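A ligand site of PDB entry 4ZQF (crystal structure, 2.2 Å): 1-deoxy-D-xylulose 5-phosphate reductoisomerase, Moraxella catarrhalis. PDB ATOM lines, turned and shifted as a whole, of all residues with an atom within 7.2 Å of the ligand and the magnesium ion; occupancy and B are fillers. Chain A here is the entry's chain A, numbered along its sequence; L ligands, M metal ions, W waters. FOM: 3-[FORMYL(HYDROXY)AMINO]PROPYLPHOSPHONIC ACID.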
ATOM      1  N   LYS A 146      15.816  22.718   2.724  1.00  0.00           N
ATOM      2  CA  LYS A 146      16.525  22.250   1.562  1.00  0.00           C
ATOM      3  C   LYS A 146      15.851  21.022   0.945  1.00  0.00           C
ATOM      4  O   LYS A 146      15.883  20.833  -0.286  1.00  0.00           O
ATOM      5  CB  LYS A 146      17.997  22.026   1.917  1.00  0.00           C
ATOM      6  CG  LYS A 146      18.663  23.264   2.531  1.00  0.00           C
ATOM      7  CD  LYS A 146      20.159  23.406   2.232  1.00  0.00           C
ATOM      8  CE  LYS A 146      20.722  24.791   2.592  1.00  0.00           C
ATOM      9  NZ  LYS A 146      19.991  25.943   1.928  1.00  0.00           N
ATOM     10  N   ILE A 170      13.987  31.688   0.736  1.00  0.00           N
ATOM     11  CA  ILE A 170      14.283  32.467   1.956  1.00  0.00           C
ATOM     12  C   ILE A 170      15.707  32.256   2.382  1.00  0.00           C
ATOM     13  O   ILE A 170      16.261  33.121   3.040  1.00  0.00           O
ATOM     14  CB  ILE A 170      13.368  31.998   3.100  1.00  0.00           C
ATOM     15  CG1 ILE A 170      12.078  32.806   3.095  1.00  0.00           C
ATOM     16  CG2 ILE A 170      14.060  32.041   4.459  1.00  0.00           C
ATOM     17  CD1 ILE A 170      11.023  32.115   3.931  1.00  0.00           C
ATOM     18  N   ASP A 171      16.287  31.107   2.064  1.00  0.00           N
ATOM     19  CA  ASP A 171      17.666  30.899   2.384  1.00  0.00           C
ATOM     20  C   ASP A 171      18.422  32.038   1.693  1.00  0.00           C
ATOM     21  O   ASP A 171      18.098  32.468   0.571  1.00  0.00           O
ATOM     22  CB  ASP A 171      18.194  29.546   1.918  1.00  0.00           C
ATOM     23  CG  ASP A 171      19.706  29.287   2.298  1.00  0.00           C
ATOM     24  OD1 ASP A 171      20.033  28.775   3.378  1.00  0.00           O
ATOM     25  OD2 ASP A 171      20.588  29.600   1.471  1.00  0.00           O
ATOM     26  N   SER A 172      19.424  32.506   2.405  1.00  0.00           N
ATOM     27  CA  SER A 172      20.167  33.717   2.074  1.00  0.00           C
ATOM     28  C   SER A 172      20.754  33.757   0.644  1.00  0.00           C
ATOM     29  O   SER A 172      20.628  34.758  -0.029  1.00  0.00           O
ATOM     30  CB  SER A 172      21.237  33.855   3.163  1.00  0.00           C
ATOM     31  OG  SER A 172      22.128  34.854   2.837  1.00  0.00           O
ATOM     32  N   GLU A 173      21.351  32.659   0.197  1.00  0.00           N
ATOM     33  CA  GLU A 173      21.957  32.560  -1.118  1.00  0.00           C
ATOM     34  C   GLU A 173      20.967  32.618  -2.242  1.00  0.00           C
ATOM     35  O   GLU A 173      21.123  33.408  -3.163  1.00  0.00           O
ATOM     36  CB  GLU A 173      22.746  31.264  -1.298  1.00  0.00           C
ATOM     37  CG  GLU A 173      24.033  31.220  -0.498  1.00  0.00           C
ATOM     38  CD  GLU A 173      23.825  30.840   0.951  1.00  0.00           C
ATOM     39  OE1 GLU A 173      24.788  30.851   1.728  1.00  0.00           O
ATOM     40  OE2 GLU A 173      22.722  30.458   1.326  1.00  0.00           O
ATOM     41  N   HIS A 174      19.959  31.774  -2.164  1.00  0.00           N
ATOM     42  CA  HIS A 174      18.951  31.715  -3.187  1.00  0.00           C
ATOM     43  C   HIS A 174      18.162  33.003  -3.289  1.00  0.00           C
ATOM     44  O   HIS A 174      17.800  33.465  -4.377  1.00  0.00           O
ATOM     45  CB  HIS A 174      18.052  30.549  -2.896  1.00  0.00           C
ATOM     46  CG  HIS A 174      18.758  29.234  -2.963  1.00  0.00           C
ATOM     47  ND1 HIS A 174      18.507  28.211  -2.071  1.00  0.00           N
ATOM     48  CD2 HIS A 174      19.755  28.805  -3.760  1.00  0.00           C
ATOM     49  CE1 HIS A 174      19.309  27.192  -2.338  1.00  0.00           C
ATOM     50  NE2 HIS A 174      20.077  27.533  -3.350  1.00  0.00           N
ATOM     51  N   THR A 205      28.083  31.839  -3.025  1.00  0.00           N
ATOM     52  CA  THR A 205      29.192  32.043  -2.085  1.00  0.00           C
ATOM     53  C   THR A 205      29.093  31.119  -0.886  1.00  0.00           C
ATOM     54  O   THR A 205      28.026  30.879  -0.364  1.00  0.00           O
ATOM     55  CB  THR A 205      29.169  33.461  -1.512  1.00  0.00           C
ATOM     56  OG1 THR A 205      27.813  33.762  -1.108  1.00  0.00           O
ATOM     57  CG2 THR A 205      29.626  34.436  -2.608  1.00  0.00           C
ATOM     58  N   ALA A 206      30.239  30.723  -0.414  1.00  0.00           N
ATOM     59  CA  ALA A 206      30.358  29.831   0.679  1.00  0.00           C
ATOM     60  C   ALA A 206      31.477  30.293   1.618  1.00  0.00           C
ATOM     61  O   ALA A 206      32.568  30.583   1.145  1.00  0.00           O
ATOM     62  CB  ALA A 206      30.680  28.435   0.101  1.00  0.00           C
ATOM     63  N   SER A 207      31.233  30.275   2.915  1.00  0.00           N
ATOM     64  CA  SER A 207      32.236  30.702   3.899  1.00  0.00           C
ATOM     65  C   SER A 207      33.435  29.803   4.018  1.00  0.00           C
ATOM     66  O   SER A 207      34.415  30.172   4.670  1.00  0.00           O
ATOM     67  CB  SER A 207      31.612  30.758   5.263  1.00  0.00           C
ATOM     68  OG  SER A 207      31.410  29.442   5.735  1.00  0.00           O
ATOM     69  N   GLY A 208      33.348  28.586   3.493  1.00  0.00           N
ATOM     70  CA  GLY A 208      34.445  27.601   3.618  1.00  0.00           C
ATOM     71  C   GLY A 208      34.465  26.902   4.972  1.00  0.00           C
ATOM     72  O   GLY A 208      35.380  26.154   5.289  1.00  0.00           O
ATOM     73  N   GLY A 209      33.455  27.142   5.785  1.00  0.00           N
ATOM     74  CA  GLY A 209      33.364  26.564   7.133  1.00  0.00           C
ATOM     75  C   GLY A 209      34.590  26.680   7.986  1.00  0.00           C
ATOM     76  O   GLY A 209      35.542  27.341   7.622  1.00  0.00           O
ATOM     77  N   SER A 210      34.585  25.987   9.131  1.00  0.00           N
ATOM     78  CA  SER A 210      35.621  26.138  10.157  1.00  0.00           C
ATOM     79  C   SER A 210      36.965  25.482   9.868  1.00  0.00           C
ATOM     80  O   SER A 210      37.889  25.598  10.672  1.00  0.00           O
ATOM     81  CB  SER A 210      35.097  25.583  11.471  1.00  0.00           C
ATOM     82  OG  SER A 210      34.616  24.263  11.288  1.00  0.00           O
ATOM     83  N   ILE A 239      23.931  21.737  10.436  1.00  0.00           N
ATOM     84  CA  ILE A 239      24.156  22.747   9.421  1.00  0.00           C
ATOM     85  C   ILE A 239      25.587  23.317   9.530  1.00  0.00           C
ATOM     86  O   ILE A 239      26.241  23.635   8.556  1.00  0.00           O
ATOM     87  CB  ILE A 239      23.014  23.797   9.498  1.00  0.00           C
ATOM     88  CG1 ILE A 239      22.751  24.440   8.124  1.00  0.00           C
ATOM     89  CG2 ILE A 239      23.253  24.800  10.626  1.00  0.00           C
ATOM     90  CD1 ILE A 239      21.743  23.672   7.288  1.00  0.00           C
ATOM     91  N   SER A 240      26.081  23.418  10.737  1.00  0.00           N
ATOM     92  CA  SER A 240      27.449  23.865  10.968  1.00  0.00           C
ATOM     93  C   SER A 240      28.484  22.815  10.470  1.00  0.00           C
ATOM     94  O   SER A 240      29.533  23.144   9.867  1.00  0.00           O
ATOM     95  CB  SER A 240      27.572  24.259  12.453  1.00  0.00           C
ATOM     96  OG  SER A 240      28.904  24.287  12.899  1.00  0.00           O
ATOM     97  N   ASP A 242      27.702  20.674   8.039  1.00  0.00           N
ATOM     98  CA  ASP A 242      27.531  20.812   6.602  1.00  0.00           C
ATOM     99  C   ASP A 242      28.337  21.990   6.018  1.00  0.00           C
ATOM    100  O   ASP A 242      28.860  21.933   4.866  1.00  0.00           O
ATOM    101  CB  ASP A 242      26.052  20.973   6.251  1.00  0.00           C
ATOM    102  CG  ASP A 242      25.259  19.632   6.335  1.00  0.00           C
ATOM    103  OD1 ASP A 242      25.849  18.568   6.593  1.00  0.00           O
ATOM    104  OD2 ASP A 242      24.042  19.676   6.134  1.00  0.00           O
ATOM    105  N   SER A 243      28.450  23.065   6.813  1.00  0.00           N
ATOM    106  CA  SER A 243      29.279  24.162   6.408  1.00  0.00           C
ATOM    107  C   SER A 243      30.724  23.719   6.414  1.00  0.00           C
ATOM    108  O   SER A 243      31.412  23.959   5.427  1.00  0.00           O
ATOM    109  CB  SER A 243      29.103  25.383   7.326  1.00  0.00           C
ATOM    110  OG  SER A 243      30.203  26.274   7.147  1.00  0.00           O
ATOM    111  N   ALA A 244      31.186  23.063   7.474  1.00  0.00           N
ATOM    112  CA  ALA A 244      32.586  22.604   7.498  1.00  0.00           C
ATOM    113  C   ALA A 244      33.030  21.582   6.426  1.00  0.00           C
ATOM    114  O   ALA A 244      34.229  21.485   6.137  1.00  0.00           O
ATOM    115  CB  ALA A 244      32.941  22.063   8.842  1.00  0.00           C
ATOM    116  N   MET A 246      31.226  21.336   3.402  1.00  0.00           N
ATOM    117  CA  MET A 246      30.758  22.009   2.226  1.00  0.00           C
ATOM    118  C   MET A 246      29.614  21.238   1.606  1.00  0.00           C
ATOM    119  O   MET A 246      29.205  21.524   0.472  1.00  0.00           O
ATOM    120  CB  MET A 246      31.882  22.226   1.228  1.00  0.00           C
ATOM    121  CG  MET A 246      31.552  23.211   0.100  1.00  0.00           C
ATOM    122  SD  MET A 246      32.083  24.916   0.313  1.00  0.00           S
ATOM    123  CE  MET A 246      33.706  24.752   1.058  1.00  0.00           C
ATOM    124  N   MET A 247      29.025  20.301   2.334  1.00  0.00           N
ATOM    125  CA  MET A 247      27.801  19.691   1.849  1.00  0.00           C
ATOM    126  C   MET A 247      26.705  20.717   1.771  1.00  0.00           C
ATOM    127  O   MET A 247      25.918  20.688   0.830  1.00  0.00           O
ATOM    128  CB  MET A 247      27.359  18.488   2.686  1.00  0.00           C
ATOM    129  CG  MET A 247      26.192  17.726   2.067  1.00  0.00           C
ATOM    130  SD  MET A 247      26.482  16.976   0.452  1.00  0.00           S
ATOM    131  CE  MET A 247      27.642  15.708   0.972  1.00  0.00           C
ATOM    132  N   ASN A 248      26.656  21.657   2.724  1.00  0.00           N
ATOM    133  CA  ASN A 248      25.605  22.723   2.611  1.00  0.00           C
ATOM    134  C   ASN A 248      25.573  23.392   1.253  1.00  0.00           C
ATOM    135  O   ASN A 248      24.497  23.627   0.686  1.00  0.00           O
ATOM    136  CB  ASN A 248      25.744  23.793   3.700  1.00  0.00           C
ATOM    137  CG  ASN A 248      24.593  24.789   3.700  1.00  0.00           C
ATOM    138  OD1 ASN A 248      23.436  24.415   3.942  1.00  0.00           O
ATOM    139  ND2 ASN A 248      24.891  26.042   3.381  1.00  0.00           N
ATOM    140  N   LYS A 249      26.754  23.710   0.720  1.00  0.00           N
ATOM    141  CA  LYS A 249      26.802  24.371  -0.596  1.00  0.00           C
ATOM    142  C   LYS A 249      26.436  23.442  -1.751  1.00  0.00           C
ATOM    143  O   LYS A 249      25.803  23.876  -2.715  1.00  0.00           O
ATOM    144  CB  LYS A 249      28.165  25.040  -0.838  1.00  0.00           C
ATOM    145  CG  LYS A 249      28.093  26.286  -1.724  1.00  0.00           C
ATOM    146  CD  LYS A 249      27.119  27.331  -1.193  1.00  0.00           C
ATOM    147  CE  LYS A 249      27.167  27.537   0.296  1.00  0.00           C
ATOM    148  NZ  LYS A 249      26.275  28.668   0.730  1.00  0.00           N
ATOM    149  N   GLY A 250      26.796  22.159  -1.650  1.00  0.00           N
ATOM    150  CA  GLY A 250      26.392  21.202  -2.693  1.00  0.00           C
ATOM    151  C   GLY A 250      24.896  21.068  -2.695  1.00  0.00           C
ATOM    152  O   GLY A 250      24.250  20.926  -3.750  1.00  0.00           O
ATOM    153  N   GLU A 252      22.792  23.365  -1.669  1.00  0.00           N
ATOM    154  CA  GLU A 252      22.308  24.609  -2.291  1.00  0.00           C
ATOM    155  C   GLU A 252      22.475  24.593  -3.814  1.00  0.00           C
ATOM    156  O   GLU A 252      21.593  24.997  -4.548  1.00  0.00           O
ATOM    157  CB  GLU A 252      22.959  25.836  -1.629  1.00  0.00           C
ATOM    158  CG  GLU A 252      22.320  26.146  -0.304  1.00  0.00           C
ATOM    159  CD  GLU A 252      23.088  27.134   0.526  1.00  0.00           C
ATOM    160  OE1 GLU A 252      24.074  27.706   0.018  1.00  0.00           O
ATOM    161  OE2 GLU A 252      22.717  27.336   1.692  1.00  0.00           O
ATOM    162  N   GLU A 255      19.540  22.573  -5.132  1.00  0.00           N
ATOM    163  CA  GLU A 255      18.322  23.386  -4.969  1.00  0.00           C
ATOM    164  C   GLU A 255      18.240  24.484  -6.013  1.00  0.00           C
ATOM    165  O   GLU A 255      17.168  24.760  -6.580  1.00  0.00           O
ATOM    166  CB  GLU A 255      18.324  24.107  -3.633  1.00  0.00           C
ATOM    167  CG  GLU A 255      17.887  23.365  -2.387  1.00  0.00           C
ATOM    168  CD  GLU A 255      17.844  24.349  -1.221  1.00  0.00           C
ATOM    169  OE1 GLU A 255      16.756  24.987  -0.948  1.00  0.00           O
ATOM    170  OE2 GLU A 255      18.947  24.557  -0.658  1.00  0.00           O
ATOM    171  N   HIS A 272      34.246  32.560   0.303  1.00  0.00           N
ATOM    172  CA  HIS A 272      34.119  33.922   0.699  1.00  0.00           C
ATOM    173  C   HIS A 272      33.896  33.891   2.192  1.00  0.00           C
ATOM    174  O   HIS A 272      32.793  33.867   2.666  1.00  0.00           O
ATOM    175  CB  HIS A 272      32.946  34.554  -0.091  1.00  0.00           C
ATOM    176  CG  HIS A 272      32.564  35.916   0.399  1.00  0.00           C
ATOM    177  ND1 HIS A 272      33.481  36.778   0.906  1.00  0.00           N
ATOM    178  CD2 HIS A 272      31.367  36.540   0.492  1.00  0.00           C
ATOM    179  CE1 HIS A 272      32.896  37.890   1.293  1.00  0.00           C
ATOM    180  NE2 HIS A 272      31.600  37.763   1.064  1.00  0.00           N
ATOM    181  N   SER A 275      31.244  35.982   4.396  1.00  0.00           N
ATOM    182  CA  SER A 275      29.806  35.872   4.116  1.00  0.00           C
ATOM    183  C   SER A 275      29.024  37.208   4.030  1.00  0.00           C
ATOM    184  O   SER A 275      27.823  37.225   4.309  1.00  0.00           O
ATOM    185  CB  SER A 275      29.118  34.951   5.121  1.00  0.00           C
ATOM    186  OG  SER A 275      29.862  33.760   5.281  1.00  0.00           O
ATOM    187  N   PRO A 295      24.168  38.478   8.451  1.00  0.00           N
ATOM    188  CA  PRO A 295      23.530  37.166   8.569  1.00  0.00           C
ATOM    189  C   PRO A 295      22.053  37.158   8.959  1.00  0.00           C
ATOM    190  O   PRO A 295      21.487  36.101   8.959  1.00  0.00           O
ATOM    191  CB  PRO A 295      24.335  36.508   9.688  1.00  0.00           C
ATOM    192  CG  PRO A 295      25.682  37.190   9.651  1.00  0.00           C
ATOM    193  CD  PRO A 295      25.344  38.595   9.336  1.00  0.00           C
ATOM    194  N   MET A 297      18.419  36.736   9.160  1.00  0.00           N
ATOM    195  CA  MET A 297      17.399  36.173   8.274  1.00  0.00           C
ATOM    196  C   MET A 297      16.199  37.026   8.084  1.00  0.00           C
ATOM    197  O   MET A 297      15.418  36.744   7.177  1.00  0.00           O
ATOM    198  CB  MET A 297      16.902  34.793   8.756  1.00  0.00           C
ATOM    199  CG  MET A 297      17.935  33.682   8.662  1.00  0.00           C
ATOM    200  SD  MET A 297      18.711  33.640   7.034  1.00  0.00           S
ATOM    201  CE  MET A 297      17.294  33.176   6.013  1.00  0.00           C
HETATM  202  O2  FOM L   1      22.777  28.151   4.740  1.00  0.00           O
HETATM  203  N1  FOM L   1      23.357  29.323   5.268  1.00  0.00           N
HETATM  204  C1  FOM L   1      22.857  30.475   5.092  1.00  0.00           C
HETATM  205  O1  FOM L   1      21.833  30.560   4.423  1.00  0.00           O
HETATM  206  C2  FOM L   1      24.607  29.221   5.999  1.00  0.00           C
HETATM  207  C3  FOM L   1      25.657  29.219   4.870  1.00  0.00           C
HETATM  208  C4  FOM L   1      26.985  28.846   5.494  1.00  0.00           C
HETATM  209  PA1 FOM L   1      28.086  28.265   4.215  1.00  0.00           P
HETATM  210  OP1 FOM L   1      29.460  27.771   4.928  1.00  0.00           O
HETATM  211  OP2 FOM L   1      28.304  29.326   3.244  1.00  0.00           O
HETATM  212  OP3 FOM L   1      27.367  27.127   3.375  1.00  0.00           O
HETATM  213 MG    MG M   1      22.154  29.065   2.886  1.00  0.00          MG
HETATM  214  O   HOH W   1      30.912  26.313   3.402  1.00  0.00           O
HETATM  215  O   HOH W   2      19.751  31.908   5.343  1.00  0.00           O
HETATM  216  O   HOH W   3      28.698  25.034   2.278  1.00  0.00           O
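The side-chain hydroxyl (OG) of Ser 207 is in hydrogen-bond range of an oxygen (OP1) of the ligand. OP1 of the ligand sits at hydrogen-bond distance from OG of Ser 243, 2.8 Å away. N of Ser 207 sits at hydrogen-bond distance from OP2 of the ligand. OP3 of the ligand lies within hydrogen-bond range of ND2 of Asn 248, 2.7 Å away. The side-chain amino group (NZ) of Lys 249 is in salt-bridge range of an oxygen (OP3) of the ligand.
Lys 146 touches the magnesium ion (NZ to MG, 3.9 Å). Four residues have an atom within 4 Å of the magnesium ion: Lys 146, Asp 171, Glu 173 and Glu 252. The nearest printed residue that does not touch the magnesium ion is Asn 248 (4.1 Å).
Water W1 lies within hydrogen-bond range of OP1 of the ligand (2.6 Å), O of Ser 243 (3.1 Å), N of Gly 208 (3.3 Å) and SD of Met 246 (3.6 Å). Water W2 bridges SD of Met 297 and N of Ser 172. Water W3 lies within hydrogen-bond range of OP3 of the ligand (2.7 Å) and N of Lys 249 (2.8 Å).
Ser 172 touches the ligand. Thr 205 touches the ligand. CA of Ala 206 touches OP2 of the ligand, at 3.3 Å. Ten residues have an atom within 4 Å of the ligand: Asp 171, Ser 172, Glu 173, Thr 205, Ala 206, Ser 207, Ser 243, Asn 248, Lys 249 and Glu 252. The nearest printed residue that does not touch the ligand is Gly 209 (4.1 Å).
The backbone carbonyl oxygen (O) of Glu 252 lies within hydrogen-bond range of a ring nitrogen (NE2) of His 174 (3.2 Å). NZ of Lys 249 is in salt-bridge range of OE1 of Glu 252, 2.5 Å away. OE2 of Glu 252 lies close to NZ of Lys 146, 3.1 Å away. OE2 of Glu 255 is in salt-bridge range of NZ of Lys 146. The side-chain carboxylate (OE2) of Glu 252 lies close to the side-chain amide nitrogen (ND2) of Asn 248 (3.0 Å). The side-chain hydroxyl of Ser 207 sits at hydrogen-bond distance from the backbone NH of Gly 209 (3.1 Å). The side-chain amino group (NZ) of Lys 249 lies within hydrogen-bond range of the backbone carbonyl oxygen (O) of Thr 205 (3.0 Å). The side-chain carboxylate (OD1) of Asp 171 sits close to the side-chain amino group (NZ) of Lys 146, at 3.2 Å.
The magnesium ion is bound by an oxygen (O2) of the ligand (2.2 Å), the side-chain carboxylate (OE2) of Glu 173 (2.2 Å), an oxygen (O1) of the ligand (2.2 Å), the side-chain carboxylate (OE2) of Glu 252 (2.2 Å), the side-chain carboxylate (OD2) of Asp 171 (2.2 Å) and the side-chain carboxylate (OD1) of Asp 171 (2.2 Å). The magnesium ion has six donor atoms within binding distance.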
